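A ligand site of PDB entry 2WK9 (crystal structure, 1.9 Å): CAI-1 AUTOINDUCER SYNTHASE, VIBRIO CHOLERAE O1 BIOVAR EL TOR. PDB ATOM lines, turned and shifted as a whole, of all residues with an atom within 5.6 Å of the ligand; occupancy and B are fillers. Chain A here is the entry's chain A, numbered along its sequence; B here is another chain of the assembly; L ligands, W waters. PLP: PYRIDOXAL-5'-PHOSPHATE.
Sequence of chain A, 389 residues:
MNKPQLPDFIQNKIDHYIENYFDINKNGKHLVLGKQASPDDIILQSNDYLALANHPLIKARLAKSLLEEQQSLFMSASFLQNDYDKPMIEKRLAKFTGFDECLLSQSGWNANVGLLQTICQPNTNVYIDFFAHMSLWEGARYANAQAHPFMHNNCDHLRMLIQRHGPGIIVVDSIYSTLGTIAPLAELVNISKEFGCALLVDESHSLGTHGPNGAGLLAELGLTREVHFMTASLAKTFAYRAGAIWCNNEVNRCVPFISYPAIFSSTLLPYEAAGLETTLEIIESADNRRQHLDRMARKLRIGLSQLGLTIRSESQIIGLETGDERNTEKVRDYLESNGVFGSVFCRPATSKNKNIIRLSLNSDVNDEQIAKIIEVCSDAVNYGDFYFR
N1 of the ligand lies within hydrogen-bond range of OD2 of Asp 202, at 2.6 Å. The backbone NH of Ser 266 of chain B lies within hydrogen-bond range of an oxygen (O1P) of the ligand (2.7 Å). N1 of the ligand lies within hydrogen-bond range of OG of Ser 204. An oxygen (O3P) of the ligand lies within hydrogen-bond range of the side-chain hydroxyl (OG) of Ser 233. An oxygen (O2P) of the ligand sits at hydrogen-bond distance from the side-chain hydroxyl (OG) of Ser 265 of chain B, 2.6 Å away. N of Gly 108 is in hydrogen-bond range of O3P of the ligand (2.7 Å). O4A of the ligand lies within hydrogen-bond range of NE2 of His 133, 3.0 Å away. An oxygen (O1P) of the ligand lies within salt-bridge range of the side-chain amino group (NZ) of Lys 236 (3.7 Å). O3 of the ligand is in hydrogen-bond range of NE2 of His 205 (2.7 Å). The backbone NH of Trp 109 sits at hydrogen-bond distance from an oxygen (O2P) of the ligand.
The side-chain carboxylate (OD1) of Asp 173 sits at hydrogen-bond distance from the backbone NH (N) of His 133, at 3.2 Å. The side-chain carboxylate (OD1) of Asp 202 lies within hydrogen-bond range of the side-chain hydroxyl (OG) of Ser 204 (2.6 Å). The backbone NH of Ser 233 lies within hydrogen-bond range of the side-chain hydroxyl of Ser 204 (2.9 Å). The backbone carbonyl oxygen of Ala 242 lies within hydrogen-bond range of the backbone NH of Leu 234. The side-chain hydroxyl (OG) of Ser 233 lies within hydrogen-bond range of the side-chain amino group (NZ) of Lys 236, at 3.3 Å. OG of Ser 135 is in hydrogen-bond range of ND2 of Asn 112, at 2.9 Å. The side-chain hydroxyl of Ser 107 sits at hydrogen-bond distance from the backbone NH of Asn 110 (3.0 Å). A ring nitrogen (ND1) of His 133 is in hydrogen-bond range of the side-chain hydroxyl (OG) of Ser 135 (2.9 Å).
The backbone carbonyl oxygen (O) of Phe 264 of chain B lies close to an oxygen (O4A) of the ligand, at 3.5 Å. Merely in contact with the ligand: Ser 107, Asn 112, Ser 135, Asp 173, Ser 177 and Ala 242. Hydrophobic or aromatic side chains within 4 Å of the ligand: Trp 109, His 133 and His 205. Within 4 Å of the ligand: Ser 107, Gly 108, Trp 109, Asn 112, His 133, Ser 135, Asp 173, Ser 177, Asp 202, Ser 204, His 205, Ser 233, Lys 236, Ala 242, Phe 264 of chain B, Ser 265 of chain B and Ser 266 of chain B.
Water W3 lies within hydrogen-bond range of O3P of the ligand (2.6 Å), OG of Ser 266 of chain B (2.8 Å) and N of Ala 242 (3.2 Å). Water W4 lies within hydrogen-bond range of an oxygen (O4A) of the ligand and a ring nitrogen (NE2) of His 133. Water W1 lies within hydrogen-bond range of the side-chain amino group (NZ) of Lys 236, an oxygen (O1P) of the ligand and the backbone NH (N) of Ser 266 of chain B. Water W2 lies within hydrogen-bond range of NH2 of Arg 358 and O4A of the ligand.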
ATOM      1  N   SER A 107     -11.642  -3.035  -1.807  1.00  0.00           N
ATOM      2  CA  SER A 107     -11.842  -2.970  -0.372  1.00  0.00           C
ATOM      3  C   SER A 107     -13.261  -2.532  -0.080  1.00  0.00           C
ATOM      4  O   SER A 107     -13.917  -1.990  -0.951  1.00  0.00           O
ATOM      5  CB  SER A 107     -10.889  -1.960   0.260  1.00  0.00           C
ATOM      6  OG  SER A 107     -11.096  -0.657  -0.279  1.00  0.00           O
ATOM      7  N   GLY A 108     -13.730  -2.768   1.141  1.00  0.00           N
ATOM      8  CA  GLY A 108     -15.030  -2.260   1.567  1.00  0.00           C
ATOM      9  C   GLY A 108     -15.047  -0.740   1.523  1.00  0.00           C
ATOM     10  O   GLY A 108     -16.064  -0.124   1.186  1.00  0.00           O
ATOM     11  N   TRP A 109     -13.921  -0.129   1.867  1.00  0.00           N
ATOM     12  CA  TRP A 109     -13.794   1.320   1.816  1.00  0.00           C
ATOM     13  C   TRP A 109     -14.086   1.824   0.398  1.00  0.00           C
ATOM     14  O   TRP A 109     -14.883   2.726   0.196  1.00  0.00           O
ATOM     15  CB  TRP A 109     -12.379   1.741   2.232  1.00  0.00           C
ATOM     16  CG  TRP A 109     -12.159   3.222   2.127  1.00  0.00           C
ATOM     17  CD1 TRP A 109     -11.875   3.930   0.993  1.00  0.00           C
ATOM     18  CD2 TRP A 109     -12.209   4.169   3.198  1.00  0.00           C
ATOM     19  NE1 TRP A 109     -11.755   5.261   1.291  1.00  0.00           N
ATOM     20  CE2 TRP A 109     -11.944   5.430   2.640  1.00  0.00           C
ATOM     21  CE3 TRP A 109     -12.428   4.062   4.568  1.00  0.00           C
ATOM     22  CZ2 TRP A 109     -11.915   6.599   3.410  1.00  0.00           C
ATOM     23  CZ3 TRP A 109     -12.406   5.216   5.340  1.00  0.00           C
ATOM     24  CH2 TRP A 109     -12.148   6.465   4.753  1.00  0.00           C
ATOM     25  N   ASN A 110     -13.406   1.233  -0.577  1.00  0.00           N
ATOM     26  CA  ASN A 110     -13.590   1.616  -1.972  1.00  0.00           C
ATOM     27  C   ASN A 110     -14.999   1.349  -2.504  1.00  0.00           C
ATOM     28  O   ASN A 110     -15.502   2.110  -3.344  1.00  0.00           O
ATOM     29  CB  ASN A 110     -12.537   0.925  -2.866  1.00  0.00           C
ATOM     30  CG  ASN A 110     -11.147   1.499  -2.680  1.00  0.00           C
ATOM     31  OD1 ASN A 110     -10.926   2.350  -1.829  1.00  0.00           O
ATOM     32  ND2 ASN A 110     -10.186   1.024  -3.491  1.00  0.00           N
ATOM     33  N   ASN A 112     -17.799   1.551  -0.799  1.00  0.00           N
ATOM     34  CA  ASN A 112     -18.627   2.647  -0.309  1.00  0.00           C
ATOM     35  C   ASN A 112     -18.326   3.984  -0.981  1.00  0.00           C
ATOM     36  O   ASN A 112     -19.238   4.700  -1.408  1.00  0.00           O
ATOM     37  CB  ASN A 112     -18.486   2.771   1.207  1.00  0.00           C
ATOM     38  CG  ASN A 112     -19.244   1.701   1.947  1.00  0.00           C
ATOM     39  OD1 ASN A 112     -20.182   1.095   1.411  1.00  0.00           O
ATOM     40  ND2 ASN A 112     -18.867   1.471   3.202  1.00  0.00           N
ATOM     41  N   HIS A 133     -20.117   3.810   9.211  1.00  0.00           N
ATOM     42  CA  HIS A 133     -18.671   3.716   9.033  1.00  0.00           C
ATOM     43  C   HIS A 133     -18.079   4.959   8.384  1.00  0.00           C
ATOM     44  O   HIS A 133     -18.721   5.606   7.558  1.00  0.00           O
ATOM     45  CB  HIS A 133     -18.307   2.484   8.212  1.00  0.00           C
ATOM     46  CG  HIS A 133     -16.857   2.117   8.314  1.00  0.00           C
ATOM     47  ND1 HIS A 133     -15.977   2.299   7.270  1.00  0.00           N
ATOM     48  CD2 HIS A 133     -16.146   1.586   9.332  1.00  0.00           C
ATOM     49  CE1 HIS A 133     -14.776   1.890   7.653  1.00  0.00           C
ATOM     50  NE2 HIS A 133     -14.852   1.452   8.886  1.00  0.00           N
ATOM     51  N   SER A 135     -15.995   5.310   6.042  1.00  0.00           N
ATOM     52  CA  SER A 135     -15.968   5.242   4.583  1.00  0.00           C
ATOM     53  C   SER A 135     -17.231   5.826   3.952  1.00  0.00           C
ATOM     54  O   SER A 135     -17.186   6.362   2.851  1.00  0.00           O
ATOM     55  CB  SER A 135     -15.736   3.789   4.097  1.00  0.00           C
ATOM     56  OG  SER A 135     -16.764   2.919   4.571  1.00  0.00           O
ATOM     57  N   ASP A 173     -25.189   1.198   8.615  1.00  0.00           N
ATOM     58  CA  ASP A 173     -24.569  -0.123   8.767  1.00  0.00           C
ATOM     59  C   ASP A 173     -25.707  -1.049   9.185  1.00  0.00           C
ATOM     60  O   ASP A 173     -26.584  -0.633   9.940  1.00  0.00           O
ATOM     61  CB  ASP A 173     -23.547  -0.124   9.908  1.00  0.00           C
ATOM     62  CG  ASP A 173     -22.274   0.677   9.618  1.00  0.00           C
ATOM     63  OD1 ASP A 173     -22.192   1.410   8.597  1.00  0.00           O
ATOM     64  OD2 ASP A 173     -21.340   0.565  10.441  1.00  0.00           O
ATOM     65  N   ILE A 175     -25.070  -3.894  10.964  1.00  0.00           N
ATOM     66  CA  ILE A 175     -24.527  -4.052  12.296  1.00  0.00           C
ATOM     67  C   ILE A 175     -23.336  -3.104  12.450  1.00  0.00           C
ATOM     68  O   ILE A 175     -22.422  -3.099  11.618  1.00  0.00           O
ATOM     69  CB  ILE A 175     -24.081  -5.497  12.558  1.00  0.00           C
ATOM     70  CG1 ILE A 175     -25.280  -6.440  12.446  1.00  0.00           C
ATOM     71  CG2 ILE A 175     -23.420  -5.610  13.934  1.00  0.00           C
ATOM     72  CD1 ILE A 175     -24.980  -7.883  12.827  1.00  0.00           C
ATOM     73  N   SER A 177     -19.993  -1.159  13.488  1.00  0.00           N
ATOM     74  CA  SER A 177     -18.662  -1.729  13.635  1.00  0.00           C
ATOM     75  C   SER A 177     -18.036  -1.492  15.011  1.00  0.00           C
ATOM     76  O   SER A 177     -17.203  -2.273  15.463  1.00  0.00           O
ATOM     77  CB  SER A 177     -17.728  -1.248  12.513  1.00  0.00           C
ATOM     78  OG  SER A 177     -17.746   0.151  12.370  1.00  0.00           O
ATOM     79  N   ASP A 202     -24.795  -1.070   4.634  1.00  0.00           N
ATOM     80  CA  ASP A 202     -23.476  -1.692   4.700  1.00  0.00           C
ATOM     81  C   ASP A 202     -23.522  -2.922   5.612  1.00  0.00           C
ATOM     82  O   ASP A 202     -23.611  -2.788   6.824  1.00  0.00           O
ATOM     83  CB  ASP A 202     -22.460  -0.673   5.218  1.00  0.00           C
ATOM     84  CG  ASP A 202     -21.037  -1.182   5.199  1.00  0.00           C
ATOM     85  OD1 ASP A 202     -20.829  -2.405   5.349  1.00  0.00           O
ATOM     86  OD2 ASP A 202     -20.114  -0.351   5.060  1.00  0.00           O
ATOM     87  N   SER A 204     -21.138  -5.220   6.149  1.00  0.00           N
ATOM     88  CA  SER A 204     -19.808  -5.742   6.442  1.00  0.00           C
ATOM     89  C   SER A 204     -19.788  -6.678   7.649  1.00  0.00           C
ATOM     90  O   SER A 204     -19.050  -7.675   7.666  1.00  0.00           O
ATOM     91  CB  SER A 204     -18.810  -4.598   6.648  1.00  0.00           C
ATOM     92  OG  SER A 204     -18.661  -3.842   5.461  1.00  0.00           O
ATOM     93  N   HIS A 205     -20.590  -6.379   8.659  1.00  0.00           N
ATOM     94  CA  HIS A 205     -20.549  -7.165   9.892  1.00  0.00           C
ATOM     95  C   HIS A 205     -21.730  -8.134  10.055  1.00  0.00           C
ATOM     96  O   HIS A 205     -21.858  -8.771  11.098  1.00  0.00           O
ATOM     97  CB  HIS A 205     -20.409  -6.247  11.103  1.00  0.00           C
ATOM     98  CG  HIS A 205     -19.172  -5.413  11.072  1.00  0.00           C
ATOM     99  ND1 HIS A 205     -17.950  -5.873  11.488  1.00  0.00           N
ATOM    100  CD2 HIS A 205     -18.968  -4.150  10.619  1.00  0.00           C
ATOM    101  CE1 HIS A 205     -17.041  -4.925  11.323  1.00  0.00           C
ATOM    102  NE2 HIS A 205     -17.638  -3.868  10.786  1.00  0.00           N
ATOM    103  N   SER A 233     -17.534  -4.939   3.080  1.00  0.00           N
ATOM    104  CA  SER A 233     -16.158  -5.379   3.114  1.00  0.00           C
ATOM    105  C   SER A 233     -16.179  -6.902   3.051  1.00  0.00           C
ATOM    106  O   SER A 233     -17.006  -7.544   3.708  1.00  0.00           O
ATOM    107  CB  SER A 233     -15.468  -4.966   4.418  1.00  0.00           C
ATOM    108  OG  SER A 233     -14.204  -5.612   4.521  1.00  0.00           O
ATOM    109  N   LEU A 234     -15.291  -7.477   2.256  1.00  0.00           N
ATOM    110  CA  LEU A 234     -15.141  -8.923   2.182  1.00  0.00           C
ATOM    111  C   LEU A 234     -14.009  -9.365   3.117  1.00  0.00           C
ATOM    112  O   LEU A 234     -13.628 -10.540   3.139  1.00  0.00           O
ATOM    113  CB  LEU A 234     -14.853  -9.343   0.742  1.00  0.00           C
ATOM    114  CG  LEU A 234     -15.980  -9.963  -0.109  1.00  0.00           C
ATOM    115  CD1 LEU A 234     -17.386  -9.686   0.412  1.00  0.00           C
ATOM    116  CD2 LEU A 234     -15.830  -9.573  -1.562  1.00  0.00           C
ATOM    117  N   ALA A 235     -13.502  -8.411   3.881  1.00  0.00           N
ATOM    118  CA  ALA A 235     -12.375  -8.626   4.781  1.00  0.00           C
ATOM    119  C   ALA A 235     -12.801  -8.974   6.208  1.00  0.00           C
ATOM    120  O   ALA A 235     -11.985  -8.977   7.130  1.00  0.00           O
ATOM    121  CB  ALA A 235     -11.448  -7.409   4.783  1.00  0.00           C
ATOM    122  N   LYS A 236     -14.077  -9.283   6.373  1.00  0.00           N
ATOM    123  CA  LYS A 236     -14.593  -9.682   7.675  1.00  0.00           C
ATOM    124  C   LYS A 236     -14.862 -11.184   7.621  1.00  0.00           C
ATOM    125  O   LYS A 236     -13.913 -11.970   7.638  1.00  0.00           O
ATOM    126  CB  LYS A 236     -15.849  -8.871   8.014  1.00  0.00           C
ATOM    127  CG  LYS A 236     -15.656  -7.355   7.877  1.00  0.00           C
ATOM    128  CD  LYS A 236     -14.573  -6.837   8.807  1.00  0.00           C
ATOM    129  CE  LYS A 236     -14.462  -5.309   8.770  1.00  0.00           C
ATOM    130  NZ  LYS A 236     -13.632  -4.834   7.637  1.00  0.00           N
ATOM    131  N   ALA A 242     -10.871  -7.207   0.074  1.00  0.00           N
ATOM    132  CA  ALA A 242     -11.660  -6.802  -1.070  1.00  0.00           C
ATOM    133  C   ALA A 242     -12.984  -6.265  -0.565  1.00  0.00           C
ATOM    134  O   ALA A 242     -13.238  -6.268   0.638  1.00  0.00           O
ATOM    135  CB  ALA A 242     -11.886  -7.967  -2.014  1.00  0.00           C
ATOM    136  N   GLY A 243     -13.824  -5.836  -1.489  1.00  0.00           N
ATOM    137  CA  GLY A 243     -15.141  -5.327  -1.160  1.00  0.00           C
ATOM    138  C   GLY A 243     -16.118  -5.615  -2.280  1.00  0.00           C
ATOM    139  O   GLY A 243     -15.728  -6.116  -3.341  1.00  0.00           O
ATOM    140  N   ARG A 358     -13.242  -2.573  21.673  1.00  0.00           N
ATOM    141  CA  ARG A 358     -14.128  -3.525  21.015  1.00  0.00           C
ATOM    142  C   ARG A 358     -13.709  -4.970  21.200  1.00  0.00           C
ATOM    143  O   ARG A 358     -12.589  -5.367  20.885  1.00  0.00           O
ATOM    144  CB  ARG A 358     -14.250  -3.201  19.523  1.00  0.00           C
ATOM    145  CG  ARG A 358     -15.136  -4.167  18.766  1.00  0.00           C
ATOM    146  CD  ARG A 358     -15.245  -3.790  17.313  1.00  0.00           C
ATOM    147  NE  ARG A 358     -14.043  -4.176  16.561  1.00  0.00           N
ATOM    148  CZ  ARG A 358     -13.859  -3.890  15.274  1.00  0.00           C
ATOM    149  NH1 ARG A 358     -14.787  -3.235  14.599  1.00  0.00           N
ATOM    150  NH2 ARG A 358     -12.749  -4.284  14.667  1.00  0.00           N
ATOM    151  N   PHE B 264      -8.830   2.760   8.494  1.00  0.00           N
ATOM    152  CA  PHE B 264     -10.187   2.263   8.346  1.00  0.00           C
ATOM    153  C   PHE B 264     -10.344   1.180   7.279  1.00  0.00           C
ATOM    154  O   PHE B 264     -11.461   0.758   6.996  1.00  0.00           O
ATOM    155  CB  PHE B 264     -11.135   3.412   8.015  1.00  0.00           C
ATOM    156  CG  PHE B 264     -11.293   4.404   9.141  1.00  0.00           C
ATOM    157  CD1 PHE B 264     -12.032   4.077  10.269  1.00  0.00           C
ATOM    158  CD2 PHE B 264     -10.691   5.657   9.072  1.00  0.00           C
ATOM    159  CE1 PHE B 264     -12.166   4.990  11.309  1.00  0.00           C
ATOM    160  CE2 PHE B 264     -10.830   6.565  10.105  1.00  0.00           C
ATOM    161  CZ  PHE B 264     -11.568   6.226  11.227  1.00  0.00           C
ATOM    162  N   SER B 265      -9.236   0.749   6.669  1.00  0.00           N
ATOM    163  CA  SER B 265      -9.298  -0.279   5.640  1.00  0.00           C
ATOM    164  C   SER B 265      -8.336  -1.413   5.993  1.00  0.00           C
ATOM    165  O   SER B 265      -7.242  -1.174   6.501  1.00  0.00           O
ATOM    166  CB  SER B 265      -8.988   0.312   4.266  1.00  0.00           C
ATOM    167  OG  SER B 265      -9.440  -0.516   3.211  1.00  0.00           O
ATOM    168  N   SER B 266      -8.737  -2.646   5.717  1.00  0.00           N
ATOM    169  CA  SER B 266      -7.972  -3.808   6.147  1.00  0.00           C
ATOM    170  C   SER B 266      -6.570  -3.842   5.553  1.00  0.00           C
ATOM    171  O   SER B 266      -6.329  -3.375   4.425  1.00  0.00           O
ATOM    172  CB  SER B 266      -8.731  -5.125   5.870  1.00  0.00           C
ATOM    173  OG  SER B 266      -8.698  -5.454   4.495  1.00  0.00           O
HETATM  174  N1  PLP L   1     -17.869  -0.785   6.302  1.00  0.00           N
HETATM  175  C2  PLP L   1     -17.824  -1.110   7.642  1.00  0.00           C
HETATM  176  C2A PLP L   1     -19.099  -1.149   8.443  1.00  0.00           C
HETATM  177  C3  PLP L   1     -16.595  -1.393   8.222  1.00  0.00           C
HETATM  178  O3  PLP L   1     -16.543  -1.716   9.556  1.00  0.00           O
HETATM  179  C4  PLP L   1     -15.425  -1.355   7.475  1.00  0.00           C
HETATM  180  C4A PLP L   1     -14.166  -1.926   8.074  1.00  0.00           C
HETATM  181  O4A PLP L   1     -13.511  -1.285   8.903  1.00  0.00           O
HETATM  182  C5  PLP L   1     -15.472  -1.010   6.124  1.00  0.00           C
HETATM  183  C6  PLP L   1     -16.701  -0.741   5.539  1.00  0.00           C
HETATM  184  C5A PLP L   1     -14.210  -0.957   5.268  1.00  0.00           C
HETATM  185  O4P PLP L   1     -13.841  -2.251   4.848  1.00  0.00           O
HETATM  186  P   PLP L   1     -12.386  -2.581   4.235  1.00  0.00           P
HETATM  187  O1P PLP L   1     -11.435  -2.842   5.372  1.00  0.00           O
HETATM  188  O2P PLP L   1     -11.941  -1.351   3.460  1.00  0.00           O
HETATM  189  O3P PLP L   1     -12.488  -3.778   3.340  1.00  0.00           O
HETATM  190  O   HOH W   1     -10.817  -3.908   8.222  1.00  0.00           O
HETATM  191  O   HOH W   2     -13.340  -3.177  11.678  1.00  0.00           O
HETATM  192  O   HOH W   3     -10.395  -4.942   2.353  1.00  0.00           O
HETATM  193  O   HOH W   4     -13.040   0.563  10.777  1.00  0.00           O
